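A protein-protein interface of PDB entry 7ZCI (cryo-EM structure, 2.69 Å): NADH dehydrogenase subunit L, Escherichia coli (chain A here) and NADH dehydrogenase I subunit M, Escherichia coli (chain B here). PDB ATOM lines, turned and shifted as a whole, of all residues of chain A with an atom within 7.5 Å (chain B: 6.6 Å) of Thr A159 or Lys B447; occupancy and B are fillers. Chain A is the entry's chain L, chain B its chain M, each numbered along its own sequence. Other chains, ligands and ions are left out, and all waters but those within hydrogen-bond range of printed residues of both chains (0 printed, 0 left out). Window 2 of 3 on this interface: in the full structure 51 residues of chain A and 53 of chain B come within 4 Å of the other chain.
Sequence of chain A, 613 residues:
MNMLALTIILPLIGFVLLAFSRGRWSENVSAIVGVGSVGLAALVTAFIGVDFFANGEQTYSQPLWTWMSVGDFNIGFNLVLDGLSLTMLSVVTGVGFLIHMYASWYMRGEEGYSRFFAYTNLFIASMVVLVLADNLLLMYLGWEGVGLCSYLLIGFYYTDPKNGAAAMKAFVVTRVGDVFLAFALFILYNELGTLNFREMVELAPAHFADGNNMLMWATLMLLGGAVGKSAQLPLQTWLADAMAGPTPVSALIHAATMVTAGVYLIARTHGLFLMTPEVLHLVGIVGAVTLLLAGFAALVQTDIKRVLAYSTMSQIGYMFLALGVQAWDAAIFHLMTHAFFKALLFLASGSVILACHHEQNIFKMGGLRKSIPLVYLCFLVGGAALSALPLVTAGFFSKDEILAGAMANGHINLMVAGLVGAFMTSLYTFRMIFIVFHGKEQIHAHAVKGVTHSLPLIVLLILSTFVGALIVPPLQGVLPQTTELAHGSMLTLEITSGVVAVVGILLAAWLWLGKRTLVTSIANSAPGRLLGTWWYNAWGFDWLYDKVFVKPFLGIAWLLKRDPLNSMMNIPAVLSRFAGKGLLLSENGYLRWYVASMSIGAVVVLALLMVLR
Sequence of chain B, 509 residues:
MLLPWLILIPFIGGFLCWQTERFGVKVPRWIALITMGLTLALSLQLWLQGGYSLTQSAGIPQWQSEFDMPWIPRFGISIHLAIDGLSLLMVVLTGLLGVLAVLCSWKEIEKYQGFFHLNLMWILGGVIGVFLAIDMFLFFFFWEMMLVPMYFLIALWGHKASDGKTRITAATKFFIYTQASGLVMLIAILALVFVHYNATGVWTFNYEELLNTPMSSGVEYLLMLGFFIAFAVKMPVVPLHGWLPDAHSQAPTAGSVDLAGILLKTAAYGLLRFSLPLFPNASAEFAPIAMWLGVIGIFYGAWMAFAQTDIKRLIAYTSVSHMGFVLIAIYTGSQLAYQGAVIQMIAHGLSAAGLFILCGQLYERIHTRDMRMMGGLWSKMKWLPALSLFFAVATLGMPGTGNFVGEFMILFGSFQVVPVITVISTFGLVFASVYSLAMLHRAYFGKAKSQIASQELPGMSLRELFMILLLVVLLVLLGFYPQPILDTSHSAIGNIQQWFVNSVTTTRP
CB of Ser B379 touches OH of Tyr A158, at 3.4 Å.
Phe B445 touches Tyr A158.
Gly B446 touches Thr A159 (O to CA, 3.7 Å).
Lys B447 touches Thr A159.
The backbone carbonyl oxygen (O) of Gly B376 sits at hydrogen-bond distance from the side-chain hydroxyl (OG) of Ser B379, 2.9 Å away.
The backbone NH of Gly B376 sits at hydrogen-bond distance from the backbone carbonyl oxygen of Phe B445 (3.4 Å).
OE1 of Glu A111 is in hydrogen-bond range of OH of Tyr A158 (2.9 Å).
Of the 12 printed residues of chain B, 4 touch a printed residue of chain A.
Hydrophobic or aromatic side chains of chain B that line the printed part of chain A: Phe B445.
Of the 11 printed residues of chain A, 2 touch a printed residue of chain B.
Hydrophobic or aromatic side chains of chain A within 4 Å of the printed part of chain B: Tyr A158.
N of Gly B446 is in hydrogen-bond range of O of Tyr A158 (2.9 Å).
Phe A156 touches none of the printed residues of chain B.
Of the printed residues of chain B, Tyr A158 touches Ser B379 (3.4 Å), Phe B445 (3.5 Å) and Gly B446 (2.9 Å).
Thr A159 touches two residues of chain B.
Asn A163 touches none of the printed residues of chain B.
Of the printed residues of chain A, Ser B379 touches Tyr A158.
Of chain A, only Thr A159 (3.4 Å) comes within 4 Å of Lys B447.
The nearest residue of chain B that does not touch Thr A159 is Phe B445 (5.8 Å).
The nearest residue of chain A that does not touch Lys B447 is Asp A160 (5.0 Å).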
ATOM      1  N   GLU A 111     -33.542  14.752 -25.177  1.00  0.00           N
ATOM      2  CA  GLU A 111     -32.650  15.041 -26.289  1.00  0.00           C
ATOM      3  C   GLU A 111     -33.100  14.266 -27.522  1.00  0.00           C
ATOM      4  O   GLU A 111     -33.488  13.099 -27.433  1.00  0.00           O
ATOM      5  CB  GLU A 111     -31.208  14.685 -25.913  1.00  0.00           C
ATOM      6  CG  GLU A 111     -30.168  14.902 -27.008  1.00  0.00           C
ATOM      7  CD  GLU A 111     -29.820  13.632 -27.777  1.00  0.00           C
ATOM      8  OE1 GLU A 111     -28.807  13.646 -28.506  1.00  0.00           O
ATOM      9  OE2 GLU A 111     -30.536  12.619 -27.639  1.00  0.00           O
ATOM     10  N   GLY A 155     -32.495   1.719 -30.654  1.00  0.00           N
ATOM     11  CA  GLY A 155     -31.298   2.282 -30.072  1.00  0.00           C
ATOM     12  C   GLY A 155     -31.329   3.793 -30.047  1.00  0.00           C
ATOM     13  O   GLY A 155     -30.338   4.442 -30.389  1.00  0.00           O
ATOM     14  N   PHE A 156     -32.469   4.362 -29.652  1.00  0.00           N
ATOM     15  CA  PHE A 156     -32.612   5.813 -29.640  1.00  0.00           C
ATOM     16  C   PHE A 156     -31.721   6.448 -28.585  1.00  0.00           C
ATOM     17  O   PHE A 156     -31.081   7.474 -28.842  1.00  0.00           O
ATOM     18  CB  PHE A 156     -34.071   6.196 -29.410  1.00  0.00           C
ATOM     19  CG  PHE A 156     -34.297   7.671 -29.355  1.00  0.00           C
ATOM     20  CD1 PHE A 156     -34.237   8.432 -30.506  1.00  0.00           C
ATOM     21  CD2 PHE A 156     -34.555   8.302 -28.155  1.00  0.00           C
ATOM     22  CE1 PHE A 156     -34.433   9.791 -30.458  1.00  0.00           C
ATOM     23  CE2 PHE A 156     -34.754   9.658 -28.103  1.00  0.00           C
ATOM     24  CZ  PHE A 156     -34.691  10.402 -29.254  1.00  0.00           C
ATOM     25  N   TYR A 157     -31.670   5.864 -27.391  1.00  0.00           N
ATOM     26  CA  TYR A 157     -30.722   6.301 -26.369  1.00  0.00           C
ATOM     27  C   TYR A 157     -29.386   5.639 -26.681  1.00  0.00           C
ATOM     28  O   TYR A 157     -29.022   4.593 -26.140  1.00  0.00           O
ATOM     29  CB  TYR A 157     -31.219   5.955 -24.974  1.00  0.00           C
ATOM     30  CG  TYR A 157     -32.571   6.534 -24.643  1.00  0.00           C
ATOM     31  CD1 TYR A 157     -32.800   7.898 -24.720  1.00  0.00           C
ATOM     32  CD2 TYR A 157     -33.615   5.714 -24.239  1.00  0.00           C
ATOM     33  CE1 TYR A 157     -34.031   8.430 -24.415  1.00  0.00           C
ATOM     34  CE2 TYR A 157     -34.851   6.241 -23.933  1.00  0.00           C
ATOM     35  CZ  TYR A 157     -35.051   7.597 -24.021  1.00  0.00           C
ATOM     36  OH  TYR A 157     -36.281   8.125 -23.715  1.00  0.00           O
ATOM     37  N   TYR A 158     -28.646   6.272 -27.592  1.00  0.00           N
ATOM     38  CA  TYR A 158     -27.422   5.690 -28.121  1.00  0.00           C
ATOM     39  C   TYR A 158     -26.277   5.714 -27.123  1.00  0.00           C
ATOM     40  O   TYR A 158     -25.283   5.012 -27.330  1.00  0.00           O
ATOM     41  CB  TYR A 158     -27.007   6.423 -29.394  1.00  0.00           C
ATOM     42  CG  TYR A 158     -26.854   7.921 -29.235  1.00  0.00           C
ATOM     43  CD1 TYR A 158     -27.923   8.776 -29.456  1.00  0.00           C
ATOM     44  CD2 TYR A 158     -25.635   8.480 -28.880  1.00  0.00           C
ATOM     45  CE1 TYR A 158     -27.789  10.135 -29.315  1.00  0.00           C
ATOM     46  CE2 TYR A 158     -25.491   9.841 -28.734  1.00  0.00           C
ATOM     47  CZ  TYR A 158     -26.571  10.664 -28.955  1.00  0.00           C
ATOM     48  OH  TYR A 158     -26.436  12.023 -28.816  1.00  0.00           O
ATOM     49  N   THR A 159     -26.388   6.512 -26.057  1.00  0.00           N
ATOM     50  CA  THR A 159     -25.316   6.619 -25.074  1.00  0.00           C
ATOM     51  C   THR A 159     -25.125   5.324 -24.297  1.00  0.00           C
ATOM     52  O   THR A 159     -23.994   4.981 -23.939  1.00  0.00           O
ATOM     53  CB  THR A 159     -25.600   7.772 -24.121  1.00  0.00           C
ATOM     54  OG1 THR A 159     -26.897   7.596 -23.541  1.00  0.00           O
ATOM     55  CG2 THR A 159     -25.568   9.088 -24.868  1.00  0.00           C
ATOM     56  N   ASP A 160     -26.201   4.604 -24.021  1.00  0.00           N
ATOM     57  CA  ASP A 160     -26.088   3.282 -23.424  1.00  0.00           C
ATOM     58  C   ASP A 160     -25.726   2.273 -24.504  1.00  0.00           C
ATOM     59  O   ASP A 160     -26.456   2.156 -25.494  1.00  0.00           O
ATOM     60  CB  ASP A 160     -27.396   2.890 -22.751  1.00  0.00           C
ATOM     61  CG  ASP A 160     -27.253   1.685 -21.837  1.00  0.00           C
ATOM     62  OD1 ASP A 160     -26.112   1.260 -21.568  1.00  0.00           O
ATOM     63  OD2 ASP A 160     -28.290   1.156 -21.386  1.00  0.00           O
ATOM     64  N   PRO A 161     -24.608   1.553 -24.378  1.00  0.00           N
ATOM     65  CA  PRO A 161     -24.266   0.545 -25.393  1.00  0.00           C
ATOM     66  C   PRO A 161     -25.210  -0.645 -25.430  1.00  0.00           C
ATOM     67  O   PRO A 161     -25.236  -1.351 -26.447  1.00  0.00           O
ATOM     68  CB  PRO A 161     -22.846   0.117 -24.999  1.00  0.00           C
ATOM     69  CG  PRO A 161     -22.326   1.241 -24.175  1.00  0.00           C
ATOM     70  CD  PRO A 161     -23.503   1.768 -23.430  1.00  0.00           C
ATOM     71  N   LYS A 162     -25.979  -0.894 -24.367  1.00  0.00           N
ATOM     72  CA  LYS A 162     -26.929  -2.002 -24.385  1.00  0.00           C
ATOM     73  C   LYS A 162     -28.053  -1.753 -25.381  1.00  0.00           C
ATOM     74  O   LYS A 162     -28.502  -2.681 -26.064  1.00  0.00           O
ATOM     75  CB  LYS A 162     -27.491  -2.233 -22.984  1.00  0.00           C
ATOM     76  CG  LYS A 162     -26.447  -2.214 -21.886  1.00  0.00           C
ATOM     77  CD  LYS A 162     -25.549  -3.440 -21.956  1.00  0.00           C
ATOM     78  CE  LYS A 162     -26.355  -4.729 -21.873  1.00  0.00           C
ATOM     79  NZ  LYS A 162     -26.387  -5.276 -20.491  1.00  0.00           N
ATOM     80  N   ASN A 163     -28.518  -0.504 -25.476  1.00  0.00           N
ATOM     81  CA  ASN A 163     -29.548  -0.156 -26.450  1.00  0.00           C
ATOM     82  C   ASN A 163     -29.038  -0.309 -27.877  1.00  0.00           C
ATOM     83  O   ASN A 163     -29.763  -0.802 -28.752  1.00  0.00           O
ATOM     84  CB  ASN A 163     -30.034   1.266 -26.197  1.00  0.00           C
ATOM     85  CG  ASN A 163     -30.277   1.534 -24.732  1.00  0.00           C
ATOM     86  OD1 ASN A 163     -30.367   0.608 -23.932  1.00  0.00           O
ATOM     87  ND2 ASN A 163     -30.382   2.802 -24.371  1.00  0.00           N
ATOM     88  N   GLY A 164     -27.791   0.094 -28.125  1.00  0.00           N
ATOM     89  CA  GLY A 164     -27.199  -0.120 -29.433  1.00  0.00           C
ATOM     90  C   GLY A 164     -27.034  -1.589 -29.771  1.00  0.00           C
ATOM     91  O   GLY A 164     -27.270  -1.999 -30.909  1.00  0.00           O
ATOM     92  N   MET B 374     -12.716   6.708 -30.125  1.00  0.00           N
ATOM     93  CA  MET B 374     -13.856   7.604 -30.230  1.00  0.00           C
ATOM     94  C   MET B 374     -15.125   6.843 -29.894  1.00  0.00           C
ATOM     95  O   MET B 374     -15.173   5.614 -29.962  1.00  0.00           O
ATOM     96  CB  MET B 374     -14.016   8.206 -31.625  1.00  0.00           C
ATOM     97  CG  MET B 374     -14.017   7.184 -32.730  1.00  0.00           C
ATOM     98  SD  MET B 374     -13.863   7.940 -34.346  1.00  0.00           S
ATOM     99  CE  MET B 374     -13.590   6.502 -35.347  1.00  0.00           C
ATOM    100  N   GLY B 375     -16.161   7.596 -29.555  1.00  0.00           N
ATOM    101  CA  GLY B 375     -17.464   7.030 -29.291  1.00  0.00           C
ATOM    102  C   GLY B 375     -18.436   8.122 -28.916  1.00  0.00           C
ATOM    103  O   GLY B 375     -18.041   9.112 -28.298  1.00  0.00           O
ATOM    104  N   GLY B 376     -19.703   7.960 -29.281  1.00  0.00           N
ATOM    105  CA  GLY B 376     -20.689   8.982 -28.984  1.00  0.00           C
ATOM    106  C   GLY B 376     -20.413  10.302 -29.666  1.00  0.00           C
ATOM    107  O   GLY B 376     -20.595  11.363 -29.057  1.00  0.00           O
ATOM    108  N   LEU B 377     -19.960  10.261 -30.914  1.00  0.00           N
ATOM    109  CA  LEU B 377     -19.698  11.483 -31.658  1.00  0.00           C
ATOM    110  C   LEU B 377     -20.955  12.068 -32.276  1.00  0.00           C
ATOM    111  O   LEU B 377     -20.878  13.129 -32.901  1.00  0.00           O
ATOM    112  CB  LEU B 377     -18.651  11.232 -32.744  1.00  0.00           C
ATOM    113  CG  LEU B 377     -17.219  10.997 -32.263  1.00  0.00           C
ATOM    114  CD1 LEU B 377     -16.336  10.603 -33.425  1.00  0.00           C
ATOM    115  CD2 LEU B 377     -16.670  12.228 -31.574  1.00  0.00           C
ATOM    116  N   SER B 379     -23.354  13.190 -30.407  1.00  0.00           N
ATOM    117  CA  SER B 379     -23.647  14.303 -29.520  1.00  0.00           C
ATOM    118  C   SER B 379     -22.668  15.456 -29.661  1.00  0.00           C
ATOM    119  O   SER B 379     -22.913  16.522 -29.089  1.00  0.00           O
ATOM    120  CB  SER B 379     -23.658  13.819 -28.071  1.00  0.00           C
ATOM    121  OG  SER B 379     -22.486  13.083 -27.779  1.00  0.00           O
ATOM    122  N   PHE B 445     -21.759   6.165 -31.856  1.00  0.00           N
ATOM    123  CA  PHE B 445     -22.695   5.868 -30.784  1.00  0.00           C
ATOM    124  C   PHE B 445     -21.958   5.315 -29.574  1.00  0.00           C
ATOM    125  O   PHE B 445     -20.864   4.757 -29.685  1.00  0.00           O
ATOM    126  CB  PHE B 445     -23.766   4.872 -31.236  1.00  0.00           C
ATOM    127  CG  PHE B 445     -24.653   5.395 -32.319  1.00  0.00           C
ATOM    128  CD1 PHE B 445     -25.058   6.714 -32.319  1.00  0.00           C
ATOM    129  CD2 PHE B 445     -25.070   4.574 -33.346  1.00  0.00           C
ATOM    130  CE1 PHE B 445     -25.871   7.199 -33.311  1.00  0.00           C
ATOM    131  CE2 PHE B 445     -25.879   5.056 -34.345  1.00  0.00           C
ATOM    132  CZ  PHE B 445     -26.279   6.372 -34.327  1.00  0.00           C
ATOM    133  N   GLY B 446     -22.579   5.476 -28.412  1.00  0.00           N
ATOM    134  CA  GLY B 446     -21.992   5.022 -27.170  1.00  0.00           C
ATOM    135  C   GLY B 446     -21.460   6.170 -26.345  1.00  0.00           C
ATOM    136  O   GLY B 446     -21.959   7.294 -26.439  1.00  0.00           O
ATOM    137  N   LYS B 447     -20.448   5.899 -25.533  1.00  0.00           N
ATOM    138  CA  LYS B 447     -19.789   6.923 -24.740  1.00  0.00           C
ATOM    139  C   LYS B 447     -18.403   7.204 -25.304  1.00  0.00           C
ATOM    140  O   LYS B 447     -17.829   6.394 -26.034  1.00  0.00           O
ATOM    141  CB  LYS B 447     -19.691   6.491 -23.275  1.00  0.00           C
ATOM    142  CG  LYS B 447     -19.947   7.607 -22.280  1.00  0.00           C
ATOM    143  CD  LYS B 447     -21.288   8.272 -22.527  1.00  0.00           C
ATOM    144  CE  LYS B 447     -22.437   7.355 -22.144  1.00  0.00           C
ATOM    145  NZ  LYS B 447     -22.430   7.018 -20.695  1.00  0.00           N
ATOM    146  N   ALA B 448     -17.870   8.372 -24.956  1.00  0.00           N
ATOM    147  CA  ALA B 448     -16.550   8.762 -25.430  1.00  0.00           C
ATOM    148  C   ALA B 448     -15.474   7.910 -24.771  1.00  0.00           C
ATOM    149  O   ALA B 448     -15.419   7.798 -23.543  1.00  0.00           O
ATOM    150  CB  ALA B 448     -16.302  10.240 -25.147  1.00  0.00           C
ATOM    151  N   LYS B 449     -14.619   7.306 -25.592  1.00  0.00           N
ATOM    152  CA  LYS B 449     -13.548   6.445 -25.114  1.00  0.00           C
ATOM    153  C   LYS B 449     -12.219   7.177 -24.984  1.00  0.00           C
ATOM    154  O   LYS B 449     -11.203   6.543 -24.683  1.00  0.00           O
ATOM    155  CB  LYS B 449     -13.392   5.240 -26.039  1.00  0.00           C
ATOM    156  CG  LYS B 449     -14.366   4.112 -25.757  1.00  0.00           C
ATOM    157  CD  LYS B 449     -14.447   3.159 -26.932  1.00  0.00           C
ATOM    158  CE  LYS B 449     -15.721   3.373 -27.722  1.00  0.00           C
ATOM    159  NZ  LYS B 449     -15.642   2.794 -29.090  1.00  0.00           N
ATOM    160  N   SER B 450     -12.202   8.487 -25.204  1.00  0.00           N
ATOM    161  CA  SER B 450     -10.979   9.273 -25.118  1.00  0.00           C
ATOM    162  C   SER B 450     -11.355  10.719 -24.835  1.00  0.00           C
ATOM    163  O   SER B 450     -12.534  11.081 -24.797  1.00  0.00           O
ATOM    164  CB  SER B 450     -10.155   9.154 -26.399  1.00  0.00           C
ATOM    165  OG  SER B 450     -10.865   9.697 -27.496  1.00  0.00           O
ATOM    166  N   ALA B 453     -12.721  12.635 -28.087  1.00  0.00           N
ATOM    167  CA  ALA B 453     -14.103  12.326 -28.431  1.00  0.00           C
ATOM    168  C   ALA B 453     -15.086  13.083 -27.549  1.00  0.00           C
ATOM    169  O   ALA B 453     -16.219  13.344 -27.969  1.00  0.00           O
ATOM    170  CB  ALA B 453     -14.344  10.823 -28.324  1.00  0.00           C
